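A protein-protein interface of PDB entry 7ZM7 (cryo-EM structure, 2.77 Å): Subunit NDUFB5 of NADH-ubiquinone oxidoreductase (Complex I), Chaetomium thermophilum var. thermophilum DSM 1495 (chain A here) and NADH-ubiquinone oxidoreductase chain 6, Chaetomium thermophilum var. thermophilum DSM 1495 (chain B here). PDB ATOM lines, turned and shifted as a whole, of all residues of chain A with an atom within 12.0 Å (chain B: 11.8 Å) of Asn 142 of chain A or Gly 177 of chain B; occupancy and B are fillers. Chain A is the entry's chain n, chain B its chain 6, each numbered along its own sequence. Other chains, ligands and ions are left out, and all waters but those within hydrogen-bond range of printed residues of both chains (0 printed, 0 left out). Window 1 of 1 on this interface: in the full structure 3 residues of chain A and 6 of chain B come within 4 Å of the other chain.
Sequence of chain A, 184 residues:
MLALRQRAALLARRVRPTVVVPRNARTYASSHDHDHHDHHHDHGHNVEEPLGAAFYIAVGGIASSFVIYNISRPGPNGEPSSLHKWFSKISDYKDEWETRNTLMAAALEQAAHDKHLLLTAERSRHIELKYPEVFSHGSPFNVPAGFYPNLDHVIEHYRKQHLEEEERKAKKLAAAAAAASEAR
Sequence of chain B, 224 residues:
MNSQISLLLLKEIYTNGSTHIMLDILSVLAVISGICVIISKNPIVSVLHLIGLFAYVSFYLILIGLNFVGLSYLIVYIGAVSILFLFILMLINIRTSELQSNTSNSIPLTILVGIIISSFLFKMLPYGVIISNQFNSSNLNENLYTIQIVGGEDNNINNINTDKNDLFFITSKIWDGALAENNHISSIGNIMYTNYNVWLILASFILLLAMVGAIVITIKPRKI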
ATOM      1  N   GLY A 138       2.679 -40.370 -13.639  1.00  0.00           N
ATOM      2  CA  GLY A 138       1.573 -39.457 -13.969  1.00  0.00           C
ATOM      3  C   GLY A 138       1.697 -38.102 -13.307  1.00  0.00           C
ATOM      4  O   GLY A 138       2.151 -38.030 -12.172  1.00  0.00           O
ATOM      5  N   SER A 139       1.324 -37.043 -14.000  1.00  0.00           N
ATOM      6  CA  SER A 139       1.389 -35.672 -13.432  1.00  0.00           C
ATOM      7  C   SER A 139       0.439 -35.498 -12.247  1.00  0.00           C
ATOM      8  O   SER A 139      -0.709 -35.911 -12.344  1.00  0.00           O
ATOM      9  CB  SER A 139       1.163 -34.619 -14.496  1.00  0.00           C
ATOM     10  OG  SER A 139       1.088 -33.321 -13.931  1.00  0.00           O
ATOM     11  N   PRO A 140       0.877 -34.872 -11.142  1.00  0.00           N
ATOM     12  CA  PRO A 140      -0.012 -34.564 -10.020  1.00  0.00           C
ATOM     13  C   PRO A 140      -0.771 -33.230 -10.162  1.00  0.00           C
ATOM     14  O   PRO A 140      -1.487 -32.890  -9.283  1.00  0.00           O
ATOM     15  CB  PRO A 140       1.008 -34.509  -8.893  1.00  0.00           C
ATOM     16  CG  PRO A 140       2.245 -33.924  -9.511  1.00  0.00           C
ATOM     17  CD  PRO A 140       2.266 -34.474 -10.916  1.00  0.00           C
ATOM     18  N   PHE A 141      -0.635 -32.546 -11.290  1.00  0.00           N
ATOM     19  CA  PHE A 141      -1.210 -31.191 -11.468  1.00  0.00           C
ATOM     20  C   PHE A 141      -2.226 -31.145 -12.596  1.00  0.00           C
ATOM     21  O   PHE A 141      -2.057 -31.905 -13.545  1.00  0.00           O
ATOM     22  CB  PHE A 141      -0.107 -30.223 -11.890  1.00  0.00           C
ATOM     23  CG  PHE A 141       1.160 -30.336 -11.085  1.00  0.00           C
ATOM     24  CD1 PHE A 141       1.154 -30.096  -9.721  1.00  0.00           C
ATOM     25  CD2 PHE A 141       2.356 -30.681 -11.690  1.00  0.00           C
ATOM     26  CE1 PHE A 141       2.314 -30.204  -8.977  1.00  0.00           C
ATOM     27  CE2 PHE A 141       3.518 -30.788 -10.944  1.00  0.00           C
ATOM     28  CZ  PHE A 141       3.490 -30.553  -9.590  1.00  0.00           C
ATOM     29  N   ASN A 142      -3.252 -30.308 -12.453  1.00  0.00           N
ATOM     30  CA  ASN A 142      -4.256 -30.086 -13.523  1.00  0.00           C
ATOM     31  C   ASN A 142      -4.911 -31.408 -13.852  1.00  0.00           C
ATOM     32  O   ASN A 142      -5.197 -31.647 -15.029  1.00  0.00           O
ATOM     33  CB  ASN A 142      -3.661 -29.326 -14.709  1.00  0.00           C
ATOM     34  CG  ASN A 142      -3.305 -27.897 -14.388  1.00  0.00           C
ATOM     35  OD1 ASN A 142      -4.048 -27.210 -13.696  1.00  0.00           O
ATOM     36  ND2 ASN A 142      -2.174 -27.448 -14.900  1.00  0.00           N
ATOM     37  N   VAL A 143      -5.135 -32.217 -12.827  1.00  0.00           N
ATOM     38  CA  VAL A 143      -5.701 -33.572 -13.033  1.00  0.00           C
ATOM     39  C   VAL A 143      -7.223 -33.460 -13.161  1.00  0.00           C
ATOM     40  O   VAL A 143      -7.833 -32.950 -12.211  1.00  0.00           O
ATOM     41  CB  VAL A 143      -5.268 -34.515 -11.902  1.00  0.00           C
ATOM     42  CG1 VAL A 143      -5.906 -35.887 -12.040  1.00  0.00           C
ATOM     43  CG2 VAL A 143      -3.759 -34.629 -11.818  1.00  0.00           C
ATOM     44  N   PRO A 144      -7.877 -33.870 -14.279  1.00  0.00           N
ATOM     45  CA  PRO A 144      -9.334 -33.847 -14.305  1.00  0.00           C
ATOM     46  C   PRO A 144      -9.985 -35.028 -13.579  1.00  0.00           C
ATOM     47  O   PRO A 144      -9.424 -36.086 -13.615  1.00  0.00           O
ATOM     48  CB  PRO A 144      -9.625 -34.068 -15.795  1.00  0.00           C
ATOM     49  CG  PRO A 144      -8.302 -33.940 -16.522  1.00  0.00           C
ATOM     50  CD  PRO A 144      -7.255 -34.335 -15.512  1.00  0.00           C
ATOM     51  N   ALA A 145     -11.090 -34.800 -12.881  1.00  0.00           N
ATOM     52  CA  ALA A 145     -11.725 -35.887 -12.103  1.00  0.00           C
ATOM     53  C   ALA A 145     -12.033 -37.076 -13.016  1.00  0.00           C
ATOM     54  O   ALA A 145     -12.600 -36.863 -14.103  1.00  0.00           O
ATOM     55  CB  ALA A 145     -12.948 -35.392 -11.385  1.00  0.00           C
ATOM     56  N   GLY A 146     -11.694 -38.280 -12.574  1.00  0.00           N
ATOM     57  CA  GLY A 146     -11.993 -39.486 -13.356  1.00  0.00           C
ATOM     58  C   GLY A 146     -10.904 -39.818 -14.341  1.00  0.00           C
ATOM     59  O   GLY A 146     -11.036 -40.841 -15.025  1.00  0.00           O
ATOM     60  N   PHE A 147      -9.873 -38.988 -14.445  1.00  0.00           N
ATOM     61  CA  PHE A 147      -8.841 -39.244 -15.474  1.00  0.00           C
ATOM     62  C   PHE A 147      -8.075 -40.509 -15.126  1.00  0.00           C
ATOM     63  O   PHE A 147      -7.947 -41.379 -15.993  1.00  0.00           O
ATOM     64  CB  PHE A 147      -7.896 -38.046 -15.582  1.00  0.00           C
ATOM     65  CG  PHE A 147      -6.714 -38.245 -16.489  1.00  0.00           C
ATOM     66  CD1 PHE A 147      -5.548 -38.820 -16.013  1.00  0.00           C
ATOM     67  CD2 PHE A 147      -6.765 -37.843 -17.812  1.00  0.00           C
ATOM     68  CE1 PHE A 147      -4.463 -39.009 -16.846  1.00  0.00           C
ATOM     69  CE2 PHE A 147      -5.673 -38.021 -18.641  1.00  0.00           C
ATOM     70  CZ  PHE A 147      -4.528 -38.598 -18.152  1.00  0.00           C
ATOM     71  N   TYR A 148      -7.639 -40.624 -13.878  1.00  0.00           N
ATOM     72  CA  TYR A 148      -6.776 -41.767 -13.491  1.00  0.00           C
ATOM     73  C   TYR A 148      -7.613 -43.004 -13.202  1.00  0.00           C
ATOM     74  O   TYR A 148      -8.666 -42.892 -12.580  1.00  0.00           O
ATOM     75  CB  TYR A 148      -5.837 -41.402 -12.346  1.00  0.00           C
ATOM     76  CG  TYR A 148      -4.645 -40.568 -12.724  1.00  0.00           C
ATOM     77  CD1 TYR A 148      -3.559 -41.126 -13.370  1.00  0.00           C
ATOM     78  CD2 TYR A 148      -4.593 -39.224 -12.410  1.00  0.00           C
ATOM     79  CE1 TYR A 148      -2.453 -40.365 -13.705  1.00  0.00           C
ATOM     80  CE2 TYR A 148      -3.495 -38.448 -12.735  1.00  0.00           C
ATOM     81  CZ  TYR A 148      -2.424 -39.021 -13.386  1.00  0.00           C
ATOM     82  OH  TYR A 148      -1.355 -38.254 -13.721  1.00  0.00           O
ATOM     83  N   SER B 172     -12.623 -28.574 -27.712  1.00  0.00           N
ATOM     84  CA  SER B 172     -13.591 -27.976 -26.756  1.00  0.00           C
ATOM     85  C   SER B 172     -12.831 -27.613 -25.479  1.00  0.00           C
ATOM     86  O   SER B 172     -11.689 -28.079 -25.334  1.00  0.00           O
ATOM     87  CB  SER B 172     -14.713 -28.923 -26.471  1.00  0.00           C
ATOM     88  OG  SER B 172     -15.541 -28.436 -25.430  1.00  0.00           O
ATOM     89  N   LYS B 173     -13.430 -26.809 -24.597  1.00  0.00           N
ATOM     90  CA  LYS B 173     -12.734 -26.333 -23.372  1.00  0.00           C
ATOM     91  C   LYS B 173     -12.828 -27.339 -22.221  1.00  0.00           C
ATOM     92  O   LYS B 173     -13.695 -28.222 -22.287  1.00  0.00           O
ATOM     93  CB  LYS B 173     -13.312 -24.974 -22.966  1.00  0.00           C
ATOM     94  CG  LYS B 173     -14.816 -24.922 -22.763  1.00  0.00           C
ATOM     95  CD  LYS B 173     -15.336 -23.540 -22.440  1.00  0.00           C
ATOM     96  CE  LYS B 173     -15.118 -22.539 -23.554  1.00  0.00           C
ATOM     97  NZ  LYS B 173     -15.714 -21.223 -23.228  1.00  0.00           N
ATOM     98  N   ILE B 174     -11.947 -27.221 -21.223  1.00  0.00           N
ATOM     99  CA  ILE B 174     -11.973 -28.077 -19.996  1.00  0.00           C
ATOM    100  C   ILE B 174     -11.712 -27.114 -18.838  1.00  0.00           C
ATOM    101  O   ILE B 174     -11.108 -26.069 -19.086  1.00  0.00           O
ATOM    102  CB  ILE B 174     -10.901 -29.184 -20.064  1.00  0.00           C
ATOM    103  CG1 ILE B 174     -11.142 -30.311 -19.060  1.00  0.00           C
ATOM    104  CG2 ILE B 174      -9.498 -28.611 -19.938  1.00  0.00           C
ATOM    105  CD1 ILE B 174      -9.997 -31.288 -18.976  1.00  0.00           C
ATOM    106  N   TRP B 175     -12.193 -27.419 -17.637  1.00  0.00           N
ATOM    107  CA  TRP B 175     -12.047 -26.458 -16.519  1.00  0.00           C
ATOM    108  C   TRP B 175     -11.160 -27.031 -15.418  1.00  0.00           C
ATOM    109  O   TRP B 175     -10.289 -26.307 -14.928  1.00  0.00           O
ATOM    110  CB  TRP B 175     -13.427 -26.041 -16.019  1.00  0.00           C
ATOM    111  CG  TRP B 175     -14.201 -25.268 -17.041  1.00  0.00           C
ATOM    112  CD1 TRP B 175     -15.186 -25.737 -17.859  1.00  0.00           C
ATOM    113  CD2 TRP B 175     -14.029 -23.881 -17.379  1.00  0.00           C
ATOM    114  NE1 TRP B 175     -15.653 -24.737 -18.664  1.00  0.00           N
ATOM    115  CE2 TRP B 175     -14.961 -23.587 -18.396  1.00  0.00           C
ATOM    116  CE3 TRP B 175     -13.187 -22.863 -16.920  1.00  0.00           C
ATOM    117  CZ2 TRP B 175     -15.073 -22.317 -18.955  1.00  0.00           C
ATOM    118  CZ3 TRP B 175     -13.301 -21.608 -17.470  1.00  0.00           C
ATOM    119  CH2 TRP B 175     -14.234 -21.341 -18.470  1.00  0.00           C
ATOM    120  N   ASP B 176     -11.357 -28.295 -15.069  1.00  0.00           N
ATOM    121  CA  ASP B 176     -10.517 -28.970 -14.043  1.00  0.00           C
ATOM    122  C   ASP B 176      -9.062 -29.029 -14.518  1.00  0.00           C
ATOM    123  O   ASP B 176      -8.170 -28.877 -13.666  1.00  0.00           O
ATOM    124  CB  ASP B 176     -11.112 -30.311 -13.598  1.00  0.00           C
ATOM    125  CG  ASP B 176     -11.684 -31.185 -14.701  1.00  0.00           C
ATOM    126  OD1 ASP B 176     -11.297 -30.995 -15.867  1.00  0.00           O
ATOM    127  OD2 ASP B 176     -12.509 -32.060 -14.377  1.00  0.00           O
ATOM    128  N   GLY B 177      -8.837 -29.238 -15.817  1.00  0.00           N
ATOM    129  CA  GLY B 177      -7.480 -29.315 -16.388  1.00  0.00           C
ATOM    130  C   GLY B 177      -6.897 -27.962 -16.758  1.00  0.00           C
ATOM    131  O   GLY B 177      -5.752 -27.935 -17.221  1.00  0.00           O
ATOM    132  N   ALA B 178      -7.651 -26.877 -16.577  1.00  0.00           N
ATOM    133  CA  ALA B 178      -7.177 -25.514 -16.913  1.00  0.00           C
ATOM    134  C   ALA B 178      -6.989 -24.669 -15.652  1.00  0.00           C
ATOM    135  O   ALA B 178      -6.904 -23.457 -15.794  1.00  0.00           O
ATOM    136  CB  ALA B 178      -8.153 -24.856 -17.854  1.00  0.00           C
ATOM    137  N   LEU B 179      -6.918 -25.282 -14.471  1.00  0.00           N
ATOM    138  CA  LEU B 179      -6.814 -24.530 -13.184  1.00  0.00           C
ATOM    139  C   LEU B 179      -5.518 -23.717 -13.144  1.00  0.00           C
ATOM    140  O   LEU B 179      -5.597 -22.493 -12.995  1.00  0.00           O
ATOM    141  CB  LEU B 179      -6.874 -25.493 -11.998  1.00  0.00           C
ATOM    142  CG  LEU B 179      -6.545 -24.889 -10.632  1.00  0.00           C
ATOM    143  CD1 LEU B 179      -7.652 -23.965 -10.157  1.00  0.00           C
ATOM    144  CD2 LEU B 179      -6.288 -25.971  -9.600  1.00  0.00           C
ATOM    145  N   ALA B 180      -4.378 -24.384 -13.307  1.00  0.00           N
ATOM    146  CA  ALA B 180      -3.078 -23.689 -13.307  1.00  0.00           C
ATOM    147  C   ALA B 180      -2.250 -24.190 -14.487  1.00  0.00           C
ATOM    148  O   ALA B 180      -1.272 -24.897 -14.263  1.00  0.00           O
ATOM    149  CB  ALA B 180      -2.392 -23.914 -11.990  1.00  0.00           C
ATOM    150  N   GLU B 181      -2.619 -23.812 -15.704  1.00  0.00           N
ATOM    151  CA  GLU B 181      -1.922 -24.295 -16.921  1.00  0.00           C
ATOM    152  C   GLU B 181      -0.475 -23.808 -16.949  1.00  0.00           C
ATOM    153  O   GLU B 181      -0.203 -22.676 -16.503  1.00  0.00           O
ATOM    154  CB  GLU B 181      -2.681 -23.897 -18.184  1.00  0.00           C
ATOM    155  CG  GLU B 181      -2.032 -24.319 -19.485  1.00  0.00           C
ATOM    156  CD  GLU B 181      -1.529 -23.177 -20.351  1.00  0.00           C
ATOM    157  OE1 GLU B 181      -1.227 -23.428 -21.534  1.00  0.00           O
ATOM    158  OE2 GLU B 181      -1.436 -22.041 -19.842  1.00  0.00           O
ATOM    159  N   ASN B 182       0.418 -24.641 -17.473  1.00  0.00           N
ATOM    160  CA  ASN B 182       1.850 -24.293 -17.487  1.00  0.00           C
ATOM    161  C   ASN B 182       2.288 -24.145 -18.935  1.00  0.00           C
ATOM    162  O   ASN B 182       1.724 -24.841 -19.789  1.00  0.00           O
ATOM    163  CB  ASN B 182       2.700 -25.339 -16.763  1.00  0.00           C
ATOM    164  CG  ASN B 182       2.257 -25.611 -15.344  1.00  0.00           C
ATOM    165  OD1 ASN B 182       1.698 -24.744 -14.678  1.00  0.00           O
ATOM    166  ND2 ASN B 182       2.514 -26.816 -14.870  1.00  0.00           N
ATOM    167  N   ASN B 183       3.228 -23.240 -19.188  1.00  0.00           N
ATOM    168  CA  ASN B 183       3.810 -23.131 -20.544  1.00  0.00           C
ATOM    169  C   ASN B 183       4.647 -24.389 -20.766  1.00  0.00           C
ATOM    170  O   ASN B 183       5.019 -25.021 -19.771  1.00  0.00           O
ATOM    171  CB  ASN B 183       4.651 -21.866 -20.669  1.00  0.00           C
ATOM    172  CG  ASN B 183       3.851 -20.602 -20.459  1.00  0.00           C
ATOM    173  OD1 ASN B 183       2.755 -20.461 -20.994  1.00  0.00           O
ATOM    174  ND2 ASN B 183       4.397 -19.674 -19.690  1.00  0.00           N
ATOM    175  N   HIS B 184       4.954 -24.730 -22.007  1.00  0.00           N
ATOM    176  CA  HIS B 184       5.690 -25.989 -22.284  1.00  0.00           C
ATOM    177  C   HIS B 184       7.015 -26.028 -21.527  1.00  0.00           C
ATOM    178  O   HIS B 184       7.393 -27.133 -21.148  1.00  0.00           O
ATOM    179  CB  HIS B 184       5.933 -26.208 -23.778  1.00  0.00           C
ATOM    180  CG  HIS B 184       4.704 -26.384 -24.602  1.00  0.00           C
ATOM    181  ND1 HIS B 184       4.648 -26.006 -25.926  1.00  0.00           N
ATOM    182  CD2 HIS B 184       3.496 -26.899 -24.307  1.00  0.00           C
ATOM    183  CE1 HIS B 184       3.457 -26.280 -26.410  1.00  0.00           C
ATOM    184  NE2 HIS B 184       2.733 -26.824 -25.438  1.00  0.00           N
ATOM    185  N   SER B 186       7.795 -24.734 -18.516  1.00  0.00           N
ATOM    186  CA  SER B 186       7.523 -25.077 -17.105  1.00  0.00           C
ATOM    187  C   SER B 186       7.150 -26.546 -16.981  1.00  0.00           C
ATOM    188  O   SER B 186       7.575 -27.159 -16.009  1.00  0.00           O
ATOM    189  CB  SER B 186       6.478 -24.171 -16.571  1.00  0.00           C
ATOM    190  OG  SER B 186       6.913 -22.822 -16.639  1.00  0.00           O
ATOM    191  N   SER B 187       6.382 -27.070 -17.928  1.00  0.00           N
ATOM    192  CA  SER B 187       6.062 -28.515 -17.942  1.00  0.00           C
ATOM    193  C   SER B 187       7.335 -29.355 -18.144  1.00  0.00           C
ATOM    194  O   SER B 187       7.460 -30.367 -17.452  1.00  0.00           O
ATOM    195  CB  SER B 187       5.010 -28.777 -18.963  1.00  0.00           C
ATOM    196  OG  SER B 187       4.017 -27.771 -18.915  1.00  0.00           O
ATOM    197  N   ILE B 188       8.239 -28.949 -19.037  1.00  0.00           N
ATOM    198  CA  ILE B 188       9.541 -29.648 -19.249  1.00  0.00           C
ATOM    199  C   ILE B 188      10.329 -29.528 -17.952  1.00  0.00           C
ATOM    200  O   ILE B 188      10.865 -30.528 -17.521  1.00  0.00           O
ATOM    201  CB  ILE B 188      10.310 -29.056 -20.454  1.00  0.00           C
ATOM    202  CG1 ILE B 188       9.580 -29.310 -21.774  1.00  0.00           C
ATOM    203  CG2 ILE B 188      11.738 -29.576 -20.506  1.00  0.00           C
ATOM    204  CD1 ILE B 188      10.182 -28.602 -22.958  1.00  0.00           C
ATOM    205  N   ASN B 190       9.238 -29.158 -14.812  1.00  0.00           N
ATOM    206  CA  ASN B 190       8.613 -29.910 -13.696  1.00  0.00           C
ATOM    207  C   ASN B 190       9.178 -31.330 -13.683  1.00  0.00           C
ATOM    208  O   ASN B 190       9.187 -31.935 -12.615  1.00  0.00           O
ATOM    209  CB  ASN B 190       7.086 -29.956 -13.794  1.00  0.00           C
ATOM    210  CG  ASN B 190       6.398 -28.618 -13.641  1.00  0.00           C
ATOM    211  OD1 ASN B 190       6.937 -27.692 -13.041  1.00  0.00           O
ATOM    212  ND2 ASN B 190       5.197 -28.508 -14.184  1.00  0.00           N
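N of Ala 145 of chain A sits at hydrogen-bond distance from OD2 of Asp 176 of chain B (3.4 Å).
ND2 of Asn 142 of chain A sits at hydrogen-bond distance from O of Ala 180 of chain B, at 2.8 Å.
Gly 138 of chain A touches none of the printed residues of chain B.
No residue of chain B comes within 4 Å of Pro 140 of chain A.
Asn 142 of chain A touches four residues of chain B.
Of the printed residues of chain B, Pro 144 of chain A touches Ile 174 (3.99 Å) and Asp 176 (3.5 Å).
Of the printed residues of chain B, Ala 145 of chain A touches Asp 176.
Phe 147 of chain A touches none of the printed residues of chain B.
Of the printed residues of chain A, Ile 174 of chain B touches Pro 144 (3.99 Å).
Asp 176 of chain B touches just these residues of chain A: Pro 144 and Ala 145.
Of chain A, only Asn 142 comes within 4 Å of Gly 177 of chain B.
Ala 178 of chain B touches none of the printed residues of chain A.
Ala 180 of chain B touches just one residue of chain A: Asn 142 (2.8 Å).
Of chain A, only Asn 142 (3.8 Å) comes within 4 Å of Glu 181 of chain B.
No residue of chain A comes within 4 Å of Asn 182 of chain B.
The nearest residue of chain A that does not touch Gly 177 of chain B is Pro 144 of chain A (4.7 Å).
The nearest printed residue of chain B that does not touch Pro 144 of chain A is Gly 177 of chain B (4.7 Å).
CA of Gly 177 of chain B touches O of Asn 142 of chain A, at 3.5 Å.
Leu 179 of chain B touches Asn 142 of chain A.
ND2 of Asn 142 of chain A touches N of Glu 181 of chain B, 3.8 Å away.
CD1 of Ile 174 of chain B touches CG of Pro 144 of chain A (3.99 Å).
Asp 176 of chain B touches Pro 144 of chain A (OD1 to CB, 3.5 Å).
The backbone carbonyl oxygen (O) of Ala 180 of chain B lies close to the side-chain amide oxygen (OD1) of Asn 182 of chain B (3.0 Å).
Of the 17 printed residues of chain B, 6 touch a printed residue of chain A.
Hydrophobic or aromatic side chains of chain B that line the printed part of chain A: Ile 174 and Leu 179.
Along chain A the printed residues that touch a printed residue of chain B span positions 142 to 145.
Among the printed residues, 7 pairs touch across the chains.
Among the printed residues, no Asp or Glu carboxylate lies within 4 Å of a Lys or Arg side-chain nitrogen of the other chain.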
